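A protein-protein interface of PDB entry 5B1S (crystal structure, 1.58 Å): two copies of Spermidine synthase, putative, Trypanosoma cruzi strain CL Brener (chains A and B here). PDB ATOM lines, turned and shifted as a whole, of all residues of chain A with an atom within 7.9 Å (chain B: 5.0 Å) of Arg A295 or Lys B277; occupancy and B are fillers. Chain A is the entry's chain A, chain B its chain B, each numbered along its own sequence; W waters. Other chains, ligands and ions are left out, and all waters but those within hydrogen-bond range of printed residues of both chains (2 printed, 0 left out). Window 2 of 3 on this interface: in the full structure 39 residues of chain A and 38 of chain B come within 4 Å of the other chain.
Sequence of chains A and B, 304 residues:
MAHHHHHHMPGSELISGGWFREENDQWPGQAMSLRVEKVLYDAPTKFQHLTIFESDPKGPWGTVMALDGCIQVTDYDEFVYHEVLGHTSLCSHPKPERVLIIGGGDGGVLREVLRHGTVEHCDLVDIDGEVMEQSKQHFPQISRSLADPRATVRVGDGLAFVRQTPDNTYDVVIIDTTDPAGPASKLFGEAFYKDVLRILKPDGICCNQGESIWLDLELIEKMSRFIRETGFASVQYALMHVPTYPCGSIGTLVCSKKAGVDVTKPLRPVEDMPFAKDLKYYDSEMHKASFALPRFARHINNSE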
ATOM      1  N   ILE A 213     -30.413  -6.362   4.419  1.00  0.00           N
ATOM      2  CA  ILE A 213     -29.192  -6.742   5.217  1.00  0.00           C
ATOM      3  C   ILE A 213     -28.217  -7.624   4.411  1.00  0.00           C
ATOM      4  O   ILE A 213     -27.025  -7.739   4.804  1.00  0.00           O
ATOM      5  CB  ILE A 213     -29.507  -7.430   6.591  1.00  0.00           C
ATOM      6  CG1 ILE A 213     -30.251  -8.771   6.351  1.00  0.00           C
ATOM      7  CG2 ILE A 213     -30.293  -6.378   7.405  1.00  0.00           C
ATOM      8  CD1 ILE A 213     -30.309  -9.600   7.613  1.00  0.00           C
ATOM      9  N   LEU A 217     -25.833  -3.728   3.358  1.00  0.00           N
ATOM     10  CA  LEU A 217     -25.567  -3.516   4.797  1.00  0.00           C
ATOM     11  C   LEU A 217     -24.796  -2.220   4.995  1.00  0.00           C
ATOM     12  O   LEU A 217     -25.074  -1.508   5.973  1.00  0.00           O
ATOM     13  CB  LEU A 217     -24.835  -4.726   5.407  1.00  0.00           C
ATOM     14  CG  LEU A 217     -24.624  -4.742   6.900  1.00  0.00           C
ATOM     15  CD1 LEU A 217     -25.912  -4.792   7.708  1.00  0.00           C
ATOM     16  CD2 LEU A 217     -23.794  -6.025   7.063  1.00  0.00           C
ATOM     17  N   ALA A 292     -34.846  -8.228  16.306  1.00  0.00           N
ATOM     18  CA  ALA A 292     -33.721  -9.188  16.508  1.00  0.00           C
ATOM     19  C   ALA A 292     -33.066  -9.444  15.213  1.00  0.00           C
ATOM     20  O   ALA A 292     -33.706  -9.892  14.260  1.00  0.00           O
ATOM     21  CB  ALA A 292     -34.275 -10.478  17.071  1.00  0.00           C
ATOM     22  N   LEU A 293     -31.802  -9.041  15.092  1.00  0.00           N
ATOM     23  CA  LEU A 293     -31.100  -9.157  13.822  1.00  0.00           C
ATOM     24  C   LEU A 293     -30.059 -10.277  13.846  1.00  0.00           C
ATOM     25  O   LEU A 293     -29.444 -10.551  14.919  1.00  0.00           O
ATOM     26  CB  LEU A 293     -30.382  -7.857  13.506  1.00  0.00           C
ATOM     27  CG  LEU A 293     -31.322  -6.621  13.500  1.00  0.00           C
ATOM     28  CD1 LEU A 293     -30.488  -5.447  12.961  1.00  0.00           C
ATOM     29  CD2 LEU A 293     -32.485  -6.829  12.481  1.00  0.00           C
ATOM     30  N   PRO A 294     -29.830 -10.928  12.742  1.00  0.00           N
ATOM     31  CA  PRO A 294     -28.686 -11.880  12.633  1.00  0.00           C
ATOM     32  C   PRO A 294     -27.359 -11.253  13.142  1.00  0.00           C
ATOM     33  O   PRO A 294     -27.145 -10.014  13.005  1.00  0.00           O
ATOM     34  CB  PRO A 294     -28.571 -12.117  11.123  1.00  0.00           C
ATOM     35  CG  PRO A 294     -29.976 -11.875  10.545  1.00  0.00           C
ATOM     36  CD  PRO A 294     -30.537 -10.773  11.449  1.00  0.00           C
ATOM     37  N   ARG A 295     -26.450 -12.055  13.755  1.00  0.00           N
ATOM     38  CA  ARG A 295     -25.201 -11.460  14.310  1.00  0.00           C
ATOM     39  C   ARG A 295     -24.517 -10.589  13.317  1.00  0.00           C
ATOM     40  O   ARG A 295     -23.967  -9.588  13.702  1.00  0.00           O
ATOM     41  CB  ARG A 295     -24.232 -12.520  14.891  1.00  0.00           C
ATOM     42  CG  ARG A 295     -24.940 -13.203  16.046  1.00  0.00           C
ATOM     43  CD  ARG A 295     -23.982 -13.894  17.022  1.00  0.00           C
ATOM     44  NE  ARG A 295     -22.635 -13.829  16.577  1.00  0.00           N
ATOM     45  CZ  ARG A 295     -21.635 -13.042  16.978  1.00  0.00           C
ATOM     46  NH1 ARG A 295     -21.632 -12.158  17.998  1.00  0.00           N
ATOM     47  NH2 ARG A 295     -20.565 -13.206  16.287  1.00  0.00           N
ATOM     48  N   PHE A 296     -24.440 -10.968  12.062  1.00  0.00           N
ATOM     49  CA  PHE A 296     -23.671 -10.182  11.070  1.00  0.00           C
ATOM     50  C   PHE A 296     -24.211  -8.774  10.831  1.00  0.00           C
ATOM     51  O   PHE A 296     -23.476  -7.903  10.340  1.00  0.00           O
ATOM     52  CB  PHE A 296     -23.503 -10.949   9.754  1.00  0.00           C
ATOM     53  CG  PHE A 296     -24.740 -10.979   8.868  1.00  0.00           C
ATOM     54  CD1 PHE A 296     -25.043  -9.881   7.992  1.00  0.00           C
ATOM     55  CD2 PHE A 296     -25.569 -12.109   8.886  1.00  0.00           C
ATOM     56  CE1 PHE A 296     -26.166  -9.959   7.141  1.00  0.00           C
ATOM     57  CE2 PHE A 296     -26.690 -12.178   8.044  1.00  0.00           C
ATOM     58  CZ  PHE A 296     -26.972 -11.115   7.166  1.00  0.00           C
ATOM     59  N   ALA A 297     -25.487  -8.547  11.193  1.00  0.00           N
ATOM     60  CA  ALA A 297     -26.196  -7.319  10.980  1.00  0.00           C
ATOM     61  C   ALA A 297     -26.431  -6.589  12.266  1.00  0.00           C
ATOM     62  O   ALA A 297     -26.974  -5.500  12.250  1.00  0.00           O
ATOM     63  CB  ALA A 297     -27.529  -7.635  10.248  1.00  0.00           C
ATOM     64  N   ARG A 298     -26.095  -7.222  13.402  1.00  0.00           N
ATOM     65  CA  ARG A 298     -26.458  -6.704  14.768  1.00  0.00           C
ATOM     66  C   ARG A 298     -25.914  -5.299  15.059  1.00  0.00           C
ATOM     67  O   ARG A 298     -26.569  -4.532  15.697  1.00  0.00           O
ATOM     68  CB  ARG A 298     -25.908  -7.674  15.828  1.00  0.00           C
ATOM     69  CG  ARG A 298     -24.394  -7.490  16.085  1.00  0.00           C
ATOM     70  CD  ARG A 298     -23.886  -8.623  16.949  1.00  0.00           C
ATOM     71  NE  ARG A 298     -22.915  -8.232  18.003  1.00  0.00           N
ATOM     72  CZ  ARG A 298     -21.570  -8.220  18.001  1.00  0.00           C
ATOM     73  NH1 ARG A 298     -20.814  -8.577  16.961  1.00  0.00           N
ATOM     74  NH2 ARG A 298     -20.944  -7.828  19.126  1.00  0.00           N
ATOM     75  N   HIS A 299     -24.766  -4.933  14.512  1.00  0.00           N
ATOM     76  CA  HIS A 299     -24.234  -3.571  14.677  1.00  0.00           C
ATOM     77  C   HIS A 299     -25.125  -2.447  14.169  1.00  0.00           C
ATOM     78  O   HIS A 299     -24.954  -1.261  14.545  1.00  0.00           O
ATOM     79  CB  HIS A 299     -22.813  -3.502  14.020  1.00  0.00           C
ATOM     80  CG  HIS A 299     -22.853  -3.720  12.564  1.00  0.00           C
ATOM     81  ND1 HIS A 299     -23.092  -4.970  11.998  1.00  0.00           N
ATOM     82  CD2 HIS A 299     -22.797  -2.843  11.549  1.00  0.00           C
ATOM     83  CE1 HIS A 299     -23.153  -4.826  10.682  1.00  0.00           C
ATOM     84  NE2 HIS A 299     -22.958  -3.542  10.383  1.00  0.00           N
ATOM     85  N   ILE A 300     -26.093  -2.741  13.299  1.00  0.00           N
ATOM     86  CA  ILE A 300     -27.052  -1.743  12.960  1.00  0.00           C
ATOM     87  C   ILE A 300     -27.809  -1.257  14.248  1.00  0.00           C
ATOM     88  O   ILE A 300     -28.076  -0.051  14.342  1.00  0.00           O
ATOM     89  CB  ILE A 300     -28.055  -2.238  11.868  1.00  0.00           C
ATOM     90  CG1 ILE A 300     -27.408  -2.673  10.511  1.00  0.00           C
ATOM     91  CG2 ILE A 300     -29.130  -1.149  11.578  1.00  0.00           C
ATOM     92  CD1 ILE A 300     -26.389  -1.682   9.897  1.00  0.00           C
ATOM     93  N   PRO B 274     -17.888 -21.082  24.336  1.00  0.00           N
ATOM     94  CA  PRO B 274     -16.733 -20.308  23.812  1.00  0.00           C
ATOM     95  C   PRO B 274     -16.737 -19.929  22.325  1.00  0.00           C
ATOM     96  O   PRO B 274     -16.044 -19.041  21.912  1.00  0.00           O
ATOM     97  CB  PRO B 274     -15.477 -21.168  24.219  1.00  0.00           C
ATOM     98  CG  PRO B 274     -16.056 -22.478  24.644  1.00  0.00           C
ATOM     99  CD  PRO B 274     -17.521 -22.375  24.957  1.00  0.00           C
ATOM    100  N   PHE B 275     -17.649 -20.548  21.551  1.00  0.00           N
ATOM    101  CA  PHE B 275     -17.712 -20.335  20.155  1.00  0.00           C
ATOM    102  C   PHE B 275     -18.874 -19.394  19.814  1.00  0.00           C
ATOM    103  O   PHE B 275     -19.070 -19.106  18.599  1.00  0.00           O
ATOM    104  CB  PHE B 275     -17.880 -21.643  19.406  1.00  0.00           C
ATOM    105  CG  PHE B 275     -19.152 -22.353  19.741  1.00  0.00           C
ATOM    106  CD1 PHE B 275     -20.413 -22.038  19.092  1.00  0.00           C
ATOM    107  CD2 PHE B 275     -19.164 -23.316  20.746  1.00  0.00           C
ATOM    108  CE1 PHE B 275     -21.561 -22.737  19.488  1.00  0.00           C
ATOM    109  CE2 PHE B 275     -20.313 -23.958  21.102  1.00  0.00           C
ATOM    110  CZ  PHE B 275     -21.546 -23.661  20.501  1.00  0.00           C
ATOM    111  N   ALA B 276     -19.633 -18.889  20.770  1.00  0.00           N
ATOM    112  CA  ALA B 276     -20.745 -17.986  20.412  1.00  0.00           C
ATOM    113  C   ALA B 276     -20.361 -16.849  19.499  1.00  0.00           C
ATOM    114  O   ALA B 276     -21.109 -16.506  18.550  1.00  0.00           O
ATOM    115  CB  ALA B 276     -21.452 -17.443  21.652  1.00  0.00           C
ATOM    116  N   LYS B 277     -19.183 -16.219  19.748  1.00  0.00           N
ATOM    117  CA  LYS B 277     -18.838 -15.089  18.914  1.00  0.00           C
ATOM    118  C   LYS B 277     -18.391 -15.383  17.462  1.00  0.00           C
ATOM    119  O   LYS B 277     -18.153 -14.448  16.678  1.00  0.00           O
ATOM    120  CB  LYS B 277     -17.797 -14.239  19.610  1.00  0.00           C
ATOM    121  CG  LYS B 277     -18.384 -13.611  20.854  1.00  0.00           C
ATOM    122  CD  LYS B 277     -17.590 -12.364  21.188  1.00  0.00           C
ATOM    123  CE  LYS B 277     -18.371 -11.159  20.696  1.00  0.00           C
ATOM    124  NZ  LYS B 277     -18.781 -10.274  21.826  1.00  0.00           N
ATOM    125  N   ASP B 278     -18.151 -16.648  17.152  1.00  0.00           N
ATOM    126  CA  ASP B 278     -17.842 -17.069  15.800  1.00  0.00           C
ATOM    127  C   ASP B 278     -19.089 -17.244  14.968  1.00  0.00           C
ATOM    128  O   ASP B 278     -18.930 -17.389  13.801  1.00  0.00           O
ATOM    129  CB  ASP B 278     -17.086 -18.364  15.835  1.00  0.00           C
ATOM    130  CG  ASP B 278     -15.752 -18.208  16.599  1.00  0.00           C
ATOM    131  OD1 ASP B 278     -15.164 -17.113  16.536  1.00  0.00           O
ATOM    132  OD2 ASP B 278     -15.388 -19.143  17.303  1.00  0.00           O
ATOM    133  N   LEU B 279     -20.276 -17.313  15.581  1.00  0.00           N
ATOM    134  CA  LEU B 279     -21.466 -17.513  14.740  1.00  0.00           C
ATOM    135  C   LEU B 279     -21.879 -16.252  14.007  1.00  0.00           C
ATOM    136  O   LEU B 279     -21.696 -15.119  14.453  1.00  0.00           O
ATOM    137  CB  LEU B 279     -22.655 -17.954  15.671  1.00  0.00           C
ATOM    138  CG  LEU B 279     -22.308 -19.220  16.484  1.00  0.00           C
ATOM    139  CD1 LEU B 279     -23.571 -19.716  17.199  1.00  0.00           C
ATOM    140  CD2 LEU B 279     -21.726 -20.331  15.620  1.00  0.00           C
ATOM    141  N   LYS B 280     -22.383 -16.486  12.790  1.00  0.00           N
ATOM    142  CA  LYS B 280     -22.769 -15.395  11.922  1.00  0.00           C
ATOM    143  C   LYS B 280     -24.263 -14.996  11.899  1.00  0.00           C
ATOM    144  O   LYS B 280     -24.632 -13.894  11.508  1.00  0.00           O
ATOM    145  CB  LYS B 280     -22.334 -15.710  10.496  1.00  0.00           C
ATOM    146  CG  LYS B 280     -20.798 -15.598  10.329  1.00  0.00           C
ATOM    147  CD  LYS B 280     -20.409 -16.387   9.063  1.00  0.00           C
ATOM    148  CE  LYS B 280     -18.880 -16.589   8.942  1.00  0.00           C
ATOM    149  NZ  LYS B 280     -18.376 -17.834   9.597  1.00  0.00           N
ATOM    150  N   TYR B 281     -25.101 -15.947  12.334  1.00  0.00           N
ATOM    151  CA  TYR B 281     -26.537 -15.663  12.384  1.00  0.00           C
ATOM    152  C   TYR B 281     -27.086 -15.832  13.821  1.00  0.00           C
ATOM    153  O   TYR B 281     -27.663 -14.860  14.348  1.00  0.00           O
ATOM    154  CB  TYR B 281     -27.257 -16.608  11.393  1.00  0.00           C
ATOM    155  CG  TYR B 281     -28.759 -16.411  11.227  1.00  0.00           C
ATOM    156  CD1 TYR B 281     -29.636 -17.082  12.037  1.00  0.00           C
ATOM    157  CD2 TYR B 281     -29.274 -15.563  10.243  1.00  0.00           C
ATOM    158  CE1 TYR B 281     -31.011 -16.916  11.836  1.00  0.00           C
ATOM    159  CE2 TYR B 281     -30.677 -15.380  10.062  1.00  0.00           C
ATOM    160  CZ  TYR B 281     -31.483 -16.082  10.886  1.00  0.00           C
ATOM    161  OH  TYR B 281     -32.844 -15.948  10.655  1.00  0.00           O
ATOM    162  N   TYR B 282     -26.928 -17.036  14.340  1.00  0.00           N
ATOM    163  CA  TYR B 282     -27.613 -17.436  15.563  1.00  0.00           C
ATOM    164  C   TYR B 282     -27.086 -16.802  16.819  1.00  0.00           C
ATOM    165  O   TYR B 282     -25.874 -16.692  17.028  1.00  0.00           O
ATOM    166  CB  TYR B 282     -27.554 -18.993  15.672  1.00  0.00           C
ATOM    167  CG  TYR B 282     -28.201 -19.524  16.923  1.00  0.00           C
ATOM    168  CD1 TYR B 282     -27.476 -19.615  18.126  1.00  0.00           C
ATOM    169  CD2 TYR B 282     -29.514 -19.948  16.874  1.00  0.00           C
ATOM    170  CE1 TYR B 282     -28.080 -20.204  19.216  1.00  0.00           C
ATOM    171  CE2 TYR B 282     -30.123 -20.469  17.965  1.00  0.00           C
ATOM    172  CZ  TYR B 282     -29.409 -20.497  19.130  1.00  0.00           C
ATOM    173  OH  TYR B 282     -29.916 -21.018  20.320  1.00  0.00           O
ATOM    174  N   ASP B 283     -28.028 -16.457  17.690  1.00  0.00           N
ATOM    175  CA  ASP B 283     -27.742 -16.110  19.124  1.00  0.00           C
ATOM    176  C   ASP B 283     -29.048 -16.225  19.877  1.00  0.00           C
ATOM    177  O   ASP B 283     -30.026 -16.684  19.304  1.00  0.00           O
ATOM    178  CB  ASP B 283     -27.048 -14.728  19.264  1.00  0.00           C
ATOM    179  CG  ASP B 283     -27.930 -13.553  18.870  1.00  0.00           C
ATOM    180  OD1 ASP B 283     -29.189 -13.607  18.774  1.00  0.00           O
ATOM    181  OD2 ASP B 283     -27.411 -12.449  18.599  1.00  0.00           O
HETATM  182  O   HOH W   1     -30.440 -11.102  17.585  1.00  0.00           O
HETATM  183  O   HOH W   2     -18.388 -11.303  16.835  1.00  0.00           O
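The backbone carbonyl oxygen (O) of Lys B277 lies within hydrogen-bond range of the guanidinium group (NH2) of Arg A295 (2.7 Å).
The guanidinium group (NE) of Arg A295 sits at hydrogen-bond distance from the backbone carbonyl oxygen (O) of Leu B279 (2.7 Å).
The backbone carbonyl oxygen of Lys B280 lies within hydrogen-bond range of the backbone NH of Arg A295 (3.4 Å).
N of Arg A295 is in hydrogen-bond range of O of Tyr B281 (3.1 Å).
The backbone NH (N) of Phe A296 sits at hydrogen-bond distance from the backbone carbonyl oxygen (O) of Lys B280 (3.0 Å).
No position is printed for both chains.
Of the 9 pairs that touch across the chains among the printed residues, none has its exchanged pair printed and touching as well.
Pro A294 touches Tyr B281 (CA to O, 3.6 Å).
Ala B276 touches Arg A295.
Tyr B282 touches Arg A295 (O to CD, 3.4 Å).
OD2 of Asp B283 touches CG of Arg A295, at 3.6 Å.
ND1 of His A299 sits close to O of Phe A296 (3.4 Å).
Of the 11 printed residues of chain A, 3 touch a printed residue of chain B.
Hydrophobic or aromatic side chains of chain A that line the printed part of chain B: Pro A294 and Phe A296.
Among the printed residues, no Asp or Glu carboxylate lies within 4 Å of a Lys or Arg side-chain nitrogen of the other chain.
Of chain B, only Ala B276 (3.7 Å), Lys B277 (2.7 Å), Leu B279 (2.7 Å), Lys B280 (3.4 Å), Tyr B281 (3.1 Å), Tyr B282 (3.4 Å) and Asp B283 (3.6 Å) come within 4 Å of Arg A295.
Lys B277 touches just one residue of chain A: Arg A295.
Printed residues of chain B within 4 Å of Phe A296: Lys B280.
Of the printed residues of chain A, Asp B283 touches Arg A295 (3.6 Å).
Printed residues of chain A within 4 Å of Lys B280: Arg A295 (3.4 Å) and Phe A296 (3.0 Å).
Printed residues of chain A within 4 Å of Tyr B281: Pro A294 (3.6 Å) and Arg A295 (3.1 Å).
Ala A297 touches none of the printed residues of chain B.
Arg A298 touches none of the printed residues of chain B.
The nearest printed residue of chain A that does not touch Asp B283 is Leu A293 (4.6 Å).
Water W1 lies within hydrogen-bond range of O of Leu A293 (2.9 Å) and OD1 of Asp B283 (3.0 Å).
Water W2 lies within hydrogen-bond range of the guanidinium group (NH2) of Arg A295 and the backbone carbonyl oxygen (O) of Lys B277.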
